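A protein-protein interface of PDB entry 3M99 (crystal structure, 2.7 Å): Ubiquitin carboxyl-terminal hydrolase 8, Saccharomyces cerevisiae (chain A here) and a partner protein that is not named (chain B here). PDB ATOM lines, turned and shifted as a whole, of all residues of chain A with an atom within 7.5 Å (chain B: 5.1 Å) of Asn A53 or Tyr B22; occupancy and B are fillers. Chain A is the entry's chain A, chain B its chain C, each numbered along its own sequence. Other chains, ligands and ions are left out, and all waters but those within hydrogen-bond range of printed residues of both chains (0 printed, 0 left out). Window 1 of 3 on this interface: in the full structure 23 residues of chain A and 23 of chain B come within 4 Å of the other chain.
Of chain A, only Phe A40, Ile A52 and Asn A53 come within 4 Å of Tyr B22.
Of the printed residues of chain B, Glu A51 touches Gln B13 (3.6 Å).
Of the printed residues of chain A, Gly B20 touches Lys A37 (3.4 Å).
Thr A57 touches none of the printed residues of chain B.
The nearest residue of chain B that does not touch Asn A53 is Gln B13 (4.7 Å).
The nearest printed residue of chain B that does not touch Glu A51 is Tyr B22 (7.3 Å).
Among the printed residues, pairs that only touch across the chains: Pro A36 with Glu B23 (3.4 Å), Phe A40 with Val B17 (3.98 Å), Phe A40 with Tyr B22 (3.9 Å), Glu A51 with Gln B13 (3.6 Å), Ile A52 with Val B17 (3.3 Å) and Ile A52 with Tyr B22 (3.7 Å).
Of the 22 printed residues of chain A, 6 touch a printed residue of chain B.
Hydrophobic or aromatic side chains of chain A within 4 Å of the printed part of chain B: Pro A36, Phe A40 and Ile A52.
Among the printed residues, 10 pairs touch across the chains.
Among the printed residues, no Asp or Glu carboxylate lies within 4 Å of a Lys or Arg side-chain nitrogen of the other chain.
The side-chain amide nitrogen of Asn A53 is in hydrogen-bond range of the side-chain hydroxyl of Tyr B22 (2.6 Å).
OE1 of Gln B13 lies close to O of Ile A52, 2.6 Å away.
The side-chain amino group of Lys A37 sits close to the backbone NH of Gly B20, 3.4 Å away.
The side-chain amino group (NZ) of Lys A37 sits close to the backbone carbonyl oxygen (O) of Val B17 (3.3 Å).
O of Met A44 sits at hydrogen-bond distance from N of Asn A53 (3.1 Å).
The backbone NH of Cys A46 sits at hydrogen-bond distance from the backbone carbonyl oxygen of Glu A51 (3.0 Å).
N of Glu A51 sits close to SG of Cys A49, 3.0 Å away.
The backbone NH (N) of Lys A45 is in hydrogen-bond range of the backbone carbonyl oxygen (O) of Phe A40, at 3.4 Å.
The backbone NH (N) of Tyr B22 is in hydrogen-bond range of the backbone carbonyl oxygen (O) of Leu B16 (2.9 Å).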
ATOM      1  N   PRO A  36     -22.441  31.766   9.278  1.00  0.00           N
ATOM      2  CA  PRO A  36     -22.746  30.914  10.427  1.00  0.00           C
ATOM      3  C   PRO A  36     -21.683  29.850  10.720  1.00  0.00           C
ATOM      4  O   PRO A  36     -21.276  29.690  11.870  1.00  0.00           O
ATOM      5  CB  PRO A  36     -24.064  30.272  10.013  1.00  0.00           C
ATOM      6  CG  PRO A  36     -24.749  31.378   9.279  1.00  0.00           C
ATOM      7  CD  PRO A  36     -23.670  32.197   8.593  1.00  0.00           C
ATOM      8  N   LYS A  37     -21.234  29.147   9.689  1.00  0.00           N
ATOM      9  CA  LYS A  37     -20.304  28.035   9.859  1.00  0.00           C
ATOM     10  C   LYS A  37     -18.944  28.497  10.388  1.00  0.00           C
ATOM     11  O   LYS A  37     -18.379  27.916  11.326  1.00  0.00           O
ATOM     12  CB  LYS A  37     -20.143  27.308   8.523  1.00  0.00           C
ATOM     13  CG  LYS A  37     -19.292  26.057   8.567  1.00  0.00           C
ATOM     14  CD  LYS A  37     -19.788  25.066   7.533  1.00  0.00           C
ATOM     15  CE  LYS A  37     -21.281  24.813   7.724  1.00  0.00           C
ATOM     16  NZ  LYS A  37     -21.763  23.644   6.936  1.00  0.00           N
ATOM     17  N   LYS A  39     -18.497  31.271  11.783  1.00  0.00           N
ATOM     18  CA  LYS A  39     -18.776  32.044  12.975  1.00  0.00           C
ATOM     19  C   LYS A  39     -18.872  31.125  14.182  1.00  0.00           C
ATOM     20  O   LYS A  39     -18.796  31.575  15.319  1.00  0.00           O
ATOM     21  CB  LYS A  39     -20.069  32.834  12.786  1.00  0.00           C
ATOM     22  CG  LYS A  39     -20.535  33.616  13.995  1.00  0.00           C
ATOM     23  CD  LYS A  39     -21.239  34.874  13.546  1.00  0.00           C
ATOM     24  CE  LYS A  39     -22.089  35.447  14.649  1.00  0.00           C
ATOM     25  NZ  LYS A  39     -21.262  35.748  15.836  1.00  0.00           N
ATOM     26  N   PHE A  40     -19.033  29.830  13.941  1.00  0.00           N
ATOM     27  CA  PHE A  40     -18.997  28.865  15.036  1.00  0.00           C
ATOM     28  C   PHE A  40     -17.572  28.361  15.313  1.00  0.00           C
ATOM     29  O   PHE A  40     -17.091  28.431  16.442  1.00  0.00           O
ATOM     30  CB  PHE A  40     -19.943  27.692  14.771  1.00  0.00           C
ATOM     31  CG  PHE A  40     -21.387  28.021  14.995  1.00  0.00           C
ATOM     32  CD1 PHE A  40     -22.323  27.844  13.987  1.00  0.00           C
ATOM     33  CD2 PHE A  40     -21.808  28.514  16.216  1.00  0.00           C
ATOM     34  CE1 PHE A  40     -23.647  28.143  14.198  1.00  0.00           C
ATOM     35  CE2 PHE A  40     -23.125  28.817  16.436  1.00  0.00           C
ATOM     36  CZ  PHE A  40     -24.050  28.634  15.427  1.00  0.00           C
ATOM     37  N   THR A  43     -15.050  31.752  16.218  1.00  0.00           N
ATOM     38  CA  THR A  43     -15.307  32.729  17.267  1.00  0.00           C
ATOM     39  C   THR A  43     -16.085  32.146  18.438  1.00  0.00           C
ATOM     40  O   THR A  43     -16.340  32.832  19.415  1.00  0.00           O
ATOM     41  CB  THR A  43     -16.072  33.935  16.719  1.00  0.00           C
ATOM     42  OG1 THR A  43     -17.394  33.527  16.357  1.00  0.00           O
ATOM     43  CG2 THR A  43     -15.366  34.515  15.493  1.00  0.00           C
ATOM     44  N   MET A  44     -16.461  30.878  18.341  1.00  0.00           N
ATOM     45  CA  MET A  44     -17.196  30.225  19.416  1.00  0.00           C
ATOM     46  C   MET A  44     -16.633  28.841  19.663  1.00  0.00           C
ATOM     47  O   MET A  44     -17.333  27.946  20.131  1.00  0.00           O
ATOM     48  CB  MET A  44     -18.678  30.123  19.069  1.00  0.00           C
ATOM     49  CG  MET A  44     -19.296  31.446  18.649  1.00  0.00           C
ATOM     50  SD  MET A  44     -21.084  31.389  18.527  1.00  0.00           S
ATOM     51  CE  MET A  44     -21.464  33.138  18.614  1.00  0.00           C
ATOM     52  N   LYS A  45     -15.364  28.678  19.312  1.00  0.00           N
ATOM     53  CA  LYS A  45     -14.602  27.487  19.635  1.00  0.00           C
ATOM     54  C   LYS A  45     -13.535  27.879  20.648  1.00  0.00           C
ATOM     55  O   LYS A  45     -12.672  28.707  20.353  1.00  0.00           O
ATOM     56  CB  LYS A  45     -13.932  26.952  18.374  1.00  0.00           C
ATOM     57  CG  LYS A  45     -13.100  25.696  18.568  1.00  0.00           C
ATOM     58  CD  LYS A  45     -12.631  25.166  17.213  1.00  0.00           C
ATOM     59  CE  LYS A  45     -12.110  23.735  17.303  1.00  0.00           C
ATOM     60  NZ  LYS A  45     -11.853  23.148  15.949  1.00  0.00           N
ATOM     61  N   CYS A  46     -13.593  27.295  21.841  1.00  0.00           N
ATOM     62  CA  CYS A  46     -12.577  27.551  22.859  1.00  0.00           C
ATOM     63  C   CYS A  46     -11.213  27.002  22.433  1.00  0.00           C
ATOM     64  O   CYS A  46     -11.100  25.846  22.012  1.00  0.00           O
ATOM     65  CB  CYS A  46     -12.989  26.937  24.198  1.00  0.00           C
ATOM     66  SG  CYS A  46     -12.049  27.539  25.623  1.00  0.00           S
ATOM     67  N   CYS A  49     -10.479  24.104  25.779  1.00  0.00           N
ATOM     68  CA  CYS A  49     -11.364  22.934  25.855  1.00  0.00           C
ATOM     69  C   CYS A  49     -11.787  22.414  24.480  1.00  0.00           C
ATOM     70  O   CYS A  49     -12.190  21.256  24.340  1.00  0.00           O
ATOM     71  CB  CYS A  49     -12.621  23.268  26.659  1.00  0.00           C
ATOM     72  SG  CYS A  49     -13.893  24.072  25.670  1.00  0.00           S
ATOM     73  N   HIS A  50     -11.717  23.287  23.481  1.00  0.00           N
ATOM     74  CA  HIS A  50     -12.083  22.945  22.110  1.00  0.00           C
ATOM     75  C   HIS A  50     -13.593  22.801  21.852  1.00  0.00           C
ATOM     76  O   HIS A  50     -14.007  22.543  20.720  1.00  0.00           O
ATOM     77  CB  HIS A  50     -11.332  21.694  21.648  1.00  0.00           C
ATOM     78  CG  HIS A  50      -9.888  21.939  21.346  1.00  0.00           C
ATOM     79  ND1 HIS A  50      -9.472  22.717  20.287  1.00  0.00           N
ATOM     80  CD2 HIS A  50      -8.757  21.505  21.962  1.00  0.00           C
ATOM     81  CE1 HIS A  50      -8.150  22.755  20.264  1.00  0.00           C
ATOM     82  NE2 HIS A  50      -7.695  22.029  21.269  1.00  0.00           N
ATOM     83  N   GLU A  51     -14.410  22.971  22.888  1.00  0.00           N
ATOM     84  CA  GLU A  51     -15.860  22.908  22.722  1.00  0.00           C
ATOM     85  C   GLU A  51     -16.381  24.186  22.067  1.00  0.00           C
ATOM     86  O   GLU A  51     -15.780  25.255  22.192  1.00  0.00           O
ATOM     87  CB  GLU A  51     -16.572  22.671  24.067  1.00  0.00           C
ATOM     88  CG  GLU A  51     -16.519  21.229  24.587  1.00  0.00           C
ATOM     89  CD  GLU A  51     -17.355  21.011  25.847  1.00  0.00           C
ATOM     90  OE1 GLU A  51     -18.605  21.095  25.771  1.00  0.00           O
ATOM     91  OE2 GLU A  51     -16.756  20.737  26.914  1.00  0.00           O
ATOM     92  N   ILE A  52     -17.496  24.075  21.357  1.00  0.00           N
ATOM     93  CA  ILE A  52     -18.139  25.256  20.814  1.00  0.00           C
ATOM     94  C   ILE A  52     -19.383  25.539  21.635  1.00  0.00           C
ATOM     95  O   ILE A  52     -20.034  24.616  22.130  1.00  0.00           O
ATOM     96  CB  ILE A  52     -18.518  25.077  19.348  1.00  0.00           C
ATOM     97  CG1 ILE A  52     -19.701  24.125  19.231  1.00  0.00           C
ATOM     98  CG2 ILE A  52     -17.322  24.572  18.534  1.00  0.00           C
ATOM     99  CD1 ILE A  52     -19.969  23.682  17.814  1.00  0.00           C
ATOM    100  N   ASN A  53     -19.701  26.819  21.790  1.00  0.00           N
ATOM    101  CA  ASN A  53     -20.782  27.241  22.669  1.00  0.00           C
ATOM    102  C   ASN A  53     -20.712  26.571  24.031  1.00  0.00           C
ATOM    103  O   ASN A  53     -21.735  26.121  24.547  1.00  0.00           O
ATOM    104  CB  ASN A  53     -22.141  26.949  22.038  1.00  0.00           C
ATOM    105  CG  ASN A  53     -22.405  27.788  20.812  1.00  0.00           C
ATOM    106  OD1 ASN A  53     -22.150  28.993  20.797  1.00  0.00           O
ATOM    107  ND2 ASN A  53     -22.926  27.157  19.773  1.00  0.00           N
ATOM    108  N   SER A  54     -19.509  26.482  24.599  1.00  0.00           N
ATOM    109  CA  SER A  54     -19.370  26.046  25.983  1.00  0.00           C
ATOM    110  C   SER A  54     -20.350  26.900  26.773  1.00  0.00           C
ATOM    111  O   SER A  54     -21.506  26.517  26.971  1.00  0.00           O
ATOM    112  CB  SER A  54     -17.944  26.250  26.489  1.00  0.00           C
ATOM    113  OG  SER A  54     -17.751  25.595  27.728  1.00  0.00           O
ATOM    114  N   GLY A  55     -19.901  28.068  27.211  1.00  0.00           N
ATOM    115  CA  GLY A  55     -20.836  29.109  27.596  1.00  0.00           C
ATOM    116  C   GLY A  55     -20.688  30.171  26.530  1.00  0.00           C
ATOM    117  O   GLY A  55     -20.502  29.851  25.354  1.00  0.00           O
ATOM    118  N   ALA A  56     -20.751  31.432  26.926  1.00  0.00           N
ATOM    119  CA  ALA A  56     -20.308  32.485  26.036  1.00  0.00           C
ATOM    120  C   ALA A  56     -18.807  32.298  25.769  1.00  0.00           C
ATOM    121  O   ALA A  56     -18.051  31.875  26.651  1.00  0.00           O
ATOM    122  CB  ALA A  56     -20.591  33.848  26.636  1.00  0.00           C
ATOM    123  N   THR A  57     -18.392  32.573  24.538  1.00  0.00           N
ATOM    124  CA  THR A  57     -16.987  32.523  24.175  1.00  0.00           C
ATOM    125  C   THR A  57     -16.510  33.946  23.914  1.00  0.00           C
ATOM    126  O   THR A  57     -17.285  34.795  23.478  1.00  0.00           O
ATOM    127  CB  THR A  57     -16.742  31.637  22.946  1.00  0.00           C
ATOM    128  OG1 THR A  57     -17.101  30.281  23.247  1.00  0.00           O
ATOM    129  CG2 THR A  57     -15.276  31.685  22.552  1.00  0.00           C
ATOM    130  N   CYS A  68     -13.802  29.914  26.324  1.00  0.00           N
ATOM    131  CA  CYS A  68     -15.167  29.718  26.799  1.00  0.00           C
ATOM    132  C   CYS A  68     -15.375  30.342  28.171  1.00  0.00           C
ATOM    133  O   CYS A  68     -14.596  31.195  28.603  1.00  0.00           O
ATOM    134  CB  CYS A  68     -15.473  28.232  26.905  1.00  0.00           C
ATOM    135  SG  CYS A  68     -14.607  27.450  28.281  1.00  0.00           S
ATOM    136  N   TRP A  69     -16.416  29.888  28.863  1.00  0.00           N
ATOM    137  CA  TRP A  69     -16.774  30.445  30.161  1.00  0.00           C
ATOM    138  C   TRP A  69     -17.152  29.382  31.196  1.00  0.00           C
ATOM    139  O   TRP A  69     -16.780  29.490  32.361  1.00  0.00           O
ATOM    140  CB  TRP A  69     -17.897  31.461  29.983  1.00  0.00           C
ATOM    141  CG  TRP A  69     -18.595  31.843  31.240  1.00  0.00           C
ATOM    142  CD1 TRP A  69     -19.493  31.093  31.936  1.00  0.00           C
ATOM    143  CD2 TRP A  69     -18.482  33.093  31.937  1.00  0.00           C
ATOM    144  NE1 TRP A  69     -19.939  31.791  33.033  1.00  0.00           N
ATOM    145  CE2 TRP A  69     -19.340  33.011  33.055  1.00  0.00           C
ATOM    146  CE3 TRP A  69     -17.743  34.254  31.723  1.00  0.00           C
ATOM    147  CZ2 TRP A  69     -19.470  34.065  33.959  1.00  0.00           C
ATOM    148  CZ3 TRP A  69     -17.878  35.293  32.621  1.00  0.00           C
ATOM    149  CH2 TRP A  69     -18.739  35.193  33.728  1.00  0.00           C
ATOM    150  N   ASN A  70     -17.887  28.358  30.771  1.00  0.00           N
ATOM    151  CA  ASN A  70     -18.315  27.291  31.677  1.00  0.00           C
ATOM    152  C   ASN A  70     -17.151  26.529  32.296  1.00  0.00           C
ATOM    153  O   ASN A  70     -17.282  25.954  33.377  1.00  0.00           O
ATOM    154  CB  ASN A  70     -19.231  26.304  30.957  1.00  0.00           C
ATOM    155  CG  ASN A  70     -20.515  26.937  30.490  1.00  0.00           C
ATOM    156  OD1 ASN A  70     -20.802  28.098  30.789  1.00  0.00           O
ATOM    157  ND2 ASN A  70     -21.306  26.173  29.757  1.00  0.00           N
ATOM    158  N   SER A  89     -18.787  36.842  21.955  1.00  0.00           N
ATOM    159  CA  SER A  89     -18.953  36.312  20.616  1.00  0.00           C
ATOM    160  C   SER A  89     -20.387  36.503  20.134  1.00  0.00           C
ATOM    161  O   SER A  89     -20.646  36.598  18.936  1.00  0.00           O
ATOM    162  CB  SER A  89     -18.591  34.829  20.645  1.00  0.00           C
ATOM    163  OG  SER A  89     -18.462  34.299  19.347  1.00  0.00           O
ATOM    164  N   ASN A  90     -21.313  36.571  21.086  1.00  0.00           N
ATOM    165  CA  ASN A  90     -22.735  36.700  20.786  1.00  0.00           C
ATOM    166  C   ASN A  90     -23.214  38.129  20.589  1.00  0.00           C
ATOM    167  O   ASN A  90     -24.283  38.334  20.027  1.00  0.00           O
ATOM    168  CB  ASN A  90     -23.588  36.056  21.884  1.00  0.00           C
ATOM    169  CG  ASN A  90     -23.430  34.551  21.944  1.00  0.00           C
ATOM    170  OD1 ASN A  90     -23.611  33.857  20.945  1.00  0.00           O
ATOM    171  ND2 ASN A  90     -23.096  34.035  23.125  1.00  0.00           N
ATOM    172  N   GLN B  13     -18.681  17.508  17.943  1.00  0.00           N
ATOM    173  CA  GLN B  13     -19.321  18.810  17.840  1.00  0.00           C
ATOM    174  C   GLN B  13     -18.907  19.431  16.511  1.00  0.00           C
ATOM    175  O   GLN B  13     -19.678  20.144  15.875  1.00  0.00           O
ATOM    176  CB  GLN B  13     -18.864  19.693  19.001  1.00  0.00           C
ATOM    177  CG  GLN B  13     -19.953  20.520  19.662  1.00  0.00           C
ATOM    178  CD  GLN B  13     -19.478  21.150  20.965  1.00  0.00           C
ATOM    179  OE1 GLN B  13     -20.049  22.128  21.445  1.00  0.00           O
ATOM    180  NE2 GLN B  13     -18.421  20.589  21.540  1.00  0.00           N
ATOM    181  N   LEU B  16     -21.199  18.279  13.477  1.00  0.00           N
ATOM    182  CA  LEU B  16     -22.484  18.964  13.488  1.00  0.00           C
ATOM    183  C   LEU B  16     -22.409  20.312  12.774  1.00  0.00           C
ATOM    184  O   LEU B  16     -23.290  20.653  11.988  1.00  0.00           O
ATOM    185  CB  LEU B  16     -23.008  19.128  14.917  1.00  0.00           C
ATOM    186  CG  LEU B  16     -24.041  18.096  15.376  1.00  0.00           C
ATOM    187  CD1 LEU B  16     -23.617  16.687  15.012  1.00  0.00           C
ATOM    188  CD2 LEU B  16     -24.278  18.213  16.863  1.00  0.00           C
ATOM    189  N   VAL B  17     -21.345  21.063  13.032  1.00  0.00           N
ATOM    190  CA  VAL B  17     -21.170  22.371  12.411  1.00  0.00           C
ATOM    191  C   VAL B  17     -20.844  22.274  10.915  1.00  0.00           C
ATOM    192  O   VAL B  17     -21.419  22.997  10.104  1.00  0.00           O
ATOM    193  CB  VAL B  17     -20.091  23.197  13.141  1.00  0.00           C
ATOM    194  CG1 VAL B  17     -19.813  24.495  12.408  1.00  0.00           C
ATOM    195  CG2 VAL B  17     -20.525  23.484  14.561  1.00  0.00           C
ATOM    196  N   GLY B  20     -23.848  21.616   8.747  1.00  0.00           N
ATOM    197  CA  GLY B  20     -24.948  22.552   8.856  1.00  0.00           C
ATOM    198  C   GLY B  20     -26.056  22.029   9.744  1.00  0.00           C
ATOM    199  O   GLY B  20     -27.160  22.573   9.762  1.00  0.00           O
ATOM    200  N   ASN B  21     -25.772  20.963  10.483  1.00  0.00           N
ATOM    201  CA  ASN B  21     -26.752  20.414  11.410  1.00  0.00           C
ATOM    202  C   ASN B  21     -26.703  21.071  12.780  1.00  0.00           C
ATOM    203  O   ASN B  21     -27.574  20.848  13.619  1.00  0.00           O
ATOM    204  CB  ASN B  21     -26.580  18.905  11.555  1.00  0.00           C
ATOM    205  CG  ASN B  21     -27.341  18.134  10.501  1.00  0.00           C
ATOM    206  OD1 ASN B  21     -27.366  18.516   9.328  1.00  0.00           O
ATOM    207  ND2 ASN B  21     -27.972  17.040  10.913  1.00  0.00           N
ATOM    208  N   TYR B  22     -25.677  21.879  13.010  1.00  0.00           N
ATOM    209  CA  TYR B  22     -25.544  22.533  14.297  1.00  0.00           C
ATOM    210  C   TYR B  22     -26.447  23.745  14.353  1.00  0.00           C
ATOM    211  O   TYR B  22     -27.129  23.973  15.351  1.00  0.00           O
ATOM    212  CB  TYR B  22     -24.103  22.952  14.568  1.00  0.00           C
ATOM    213  CG  TYR B  22     -23.884  23.387  16.001  1.00  0.00           C
ATOM    214  CD1 TYR B  22     -23.699  22.449  17.009  1.00  0.00           C
ATOM    215  CD2 TYR B  22     -23.879  24.732  16.349  1.00  0.00           C
ATOM    216  CE1 TYR B  22     -23.506  22.836  18.316  1.00  0.00           C
ATOM    217  CE2 TYR B  22     -23.685  25.126  17.652  1.00  0.00           C
ATOM    218  CZ  TYR B  22     -23.499  24.174  18.634  1.00  0.00           C
ATOM    219  OH  TYR B  22     -23.306  24.562  19.943  1.00  0.00           O
ATOM    220  N   GLU B  23     -26.455  24.521  13.278  1.00  0.00           N
ATOM    221  CA  GLU B  23     -27.289  25.710  13.238  1.00  0.00           C
ATOM    222  C   GLU B  23     -28.757  25.309  13.115  1.00  0.00           C
ATOM    223  O   GLU B  23     -29.654  26.022  13.570  1.00  0.00           O
ATOM    224  CB  GLU B  23     -26.854  26.652  12.114  1.00  0.00           C
ATOM    225  CG  GLU B  23     -27.414  26.326  10.755  1.00  0.00           C
ATOM    226  CD  GLU B  23     -26.746  27.136   9.663  1.00  0.00           C
ATOM    227  OE1 GLU B  23     -25.494  27.165   9.635  1.00  0.00           O
ATOM    228  OE2 GLU B  23     -27.467  27.739   8.838  1.00  0.00           O
ATOM    229  N   LEU B  24     -28.994  24.144  12.528  1.00  0.00           N
ATOM    230  CA  LEU B  24     -30.342  23.614  12.453  1.00  0.00           C
ATOM    231  C   LEU B  24     -30.903  23.422  13.857  1.00  0.00           C
ATOM    232  O   LEU B  24     -32.099  23.594  14.088  1.00  0.00           O
ATOM    233  CB  LEU B  24     -30.356  22.284  11.707  1.00  0.00           C
ATOM    234  CG  LEU B  24     -31.592  22.073  10.836  1.00  0.00           C
ATOM    235  CD1 LEU B  24     -31.342  22.655   9.448  1.00  0.00           C
ATOM    236  CD2 LEU B  24     -31.967  20.600  10.755  1.00  0.00           C
ATOM    237  N   ILE B  25     -30.036  23.070  14.800  1.00  0.00           N
ATOM    238  CA  ILE B  25     -30.483  22.777  16.156  1.00  0.00           C
ATOM    239  C   ILE B  25     -30.570  24.025  17.014  1.00  0.00           C
ATOM    240  O   ILE B  25     -31.437  24.128  17.879  1.00  0.00           O
ATOM    241  CB  ILE B  25     -29.580  21.758  16.845  1.00  0.00           C
ATOM    242  CG1 ILE B  25     -29.545  20.466  16.035  1.00  0.00           C
ATOM    243  CG2 ILE B  25     -30.087  21.478  18.245  1.00  0.00           C
ATOM    244  CD1 ILE B  25     -28.436  19.533  16.432  1.00  0.00           C
ATOM    245  N   SER B  26     -29.668  24.970  16.775  1.00  0.00           N
ATOM    246  CA  SER B  26     -29.693  26.232  17.498  1.00  0.00           C
ATOM    247  C   SER B  26     -30.978  26.966  17.198  1.00  0.00           C
ATOM    248  O   SER B  26     -31.686  27.410  18.108  1.00  0.00           O
ATOM    249  CB  SER B  26     -28.520  27.111  17.092  1.00  0.00           C
ATOM    250  OG  SER B  26     -27.405  26.856  17.916  1.00  0.00           O
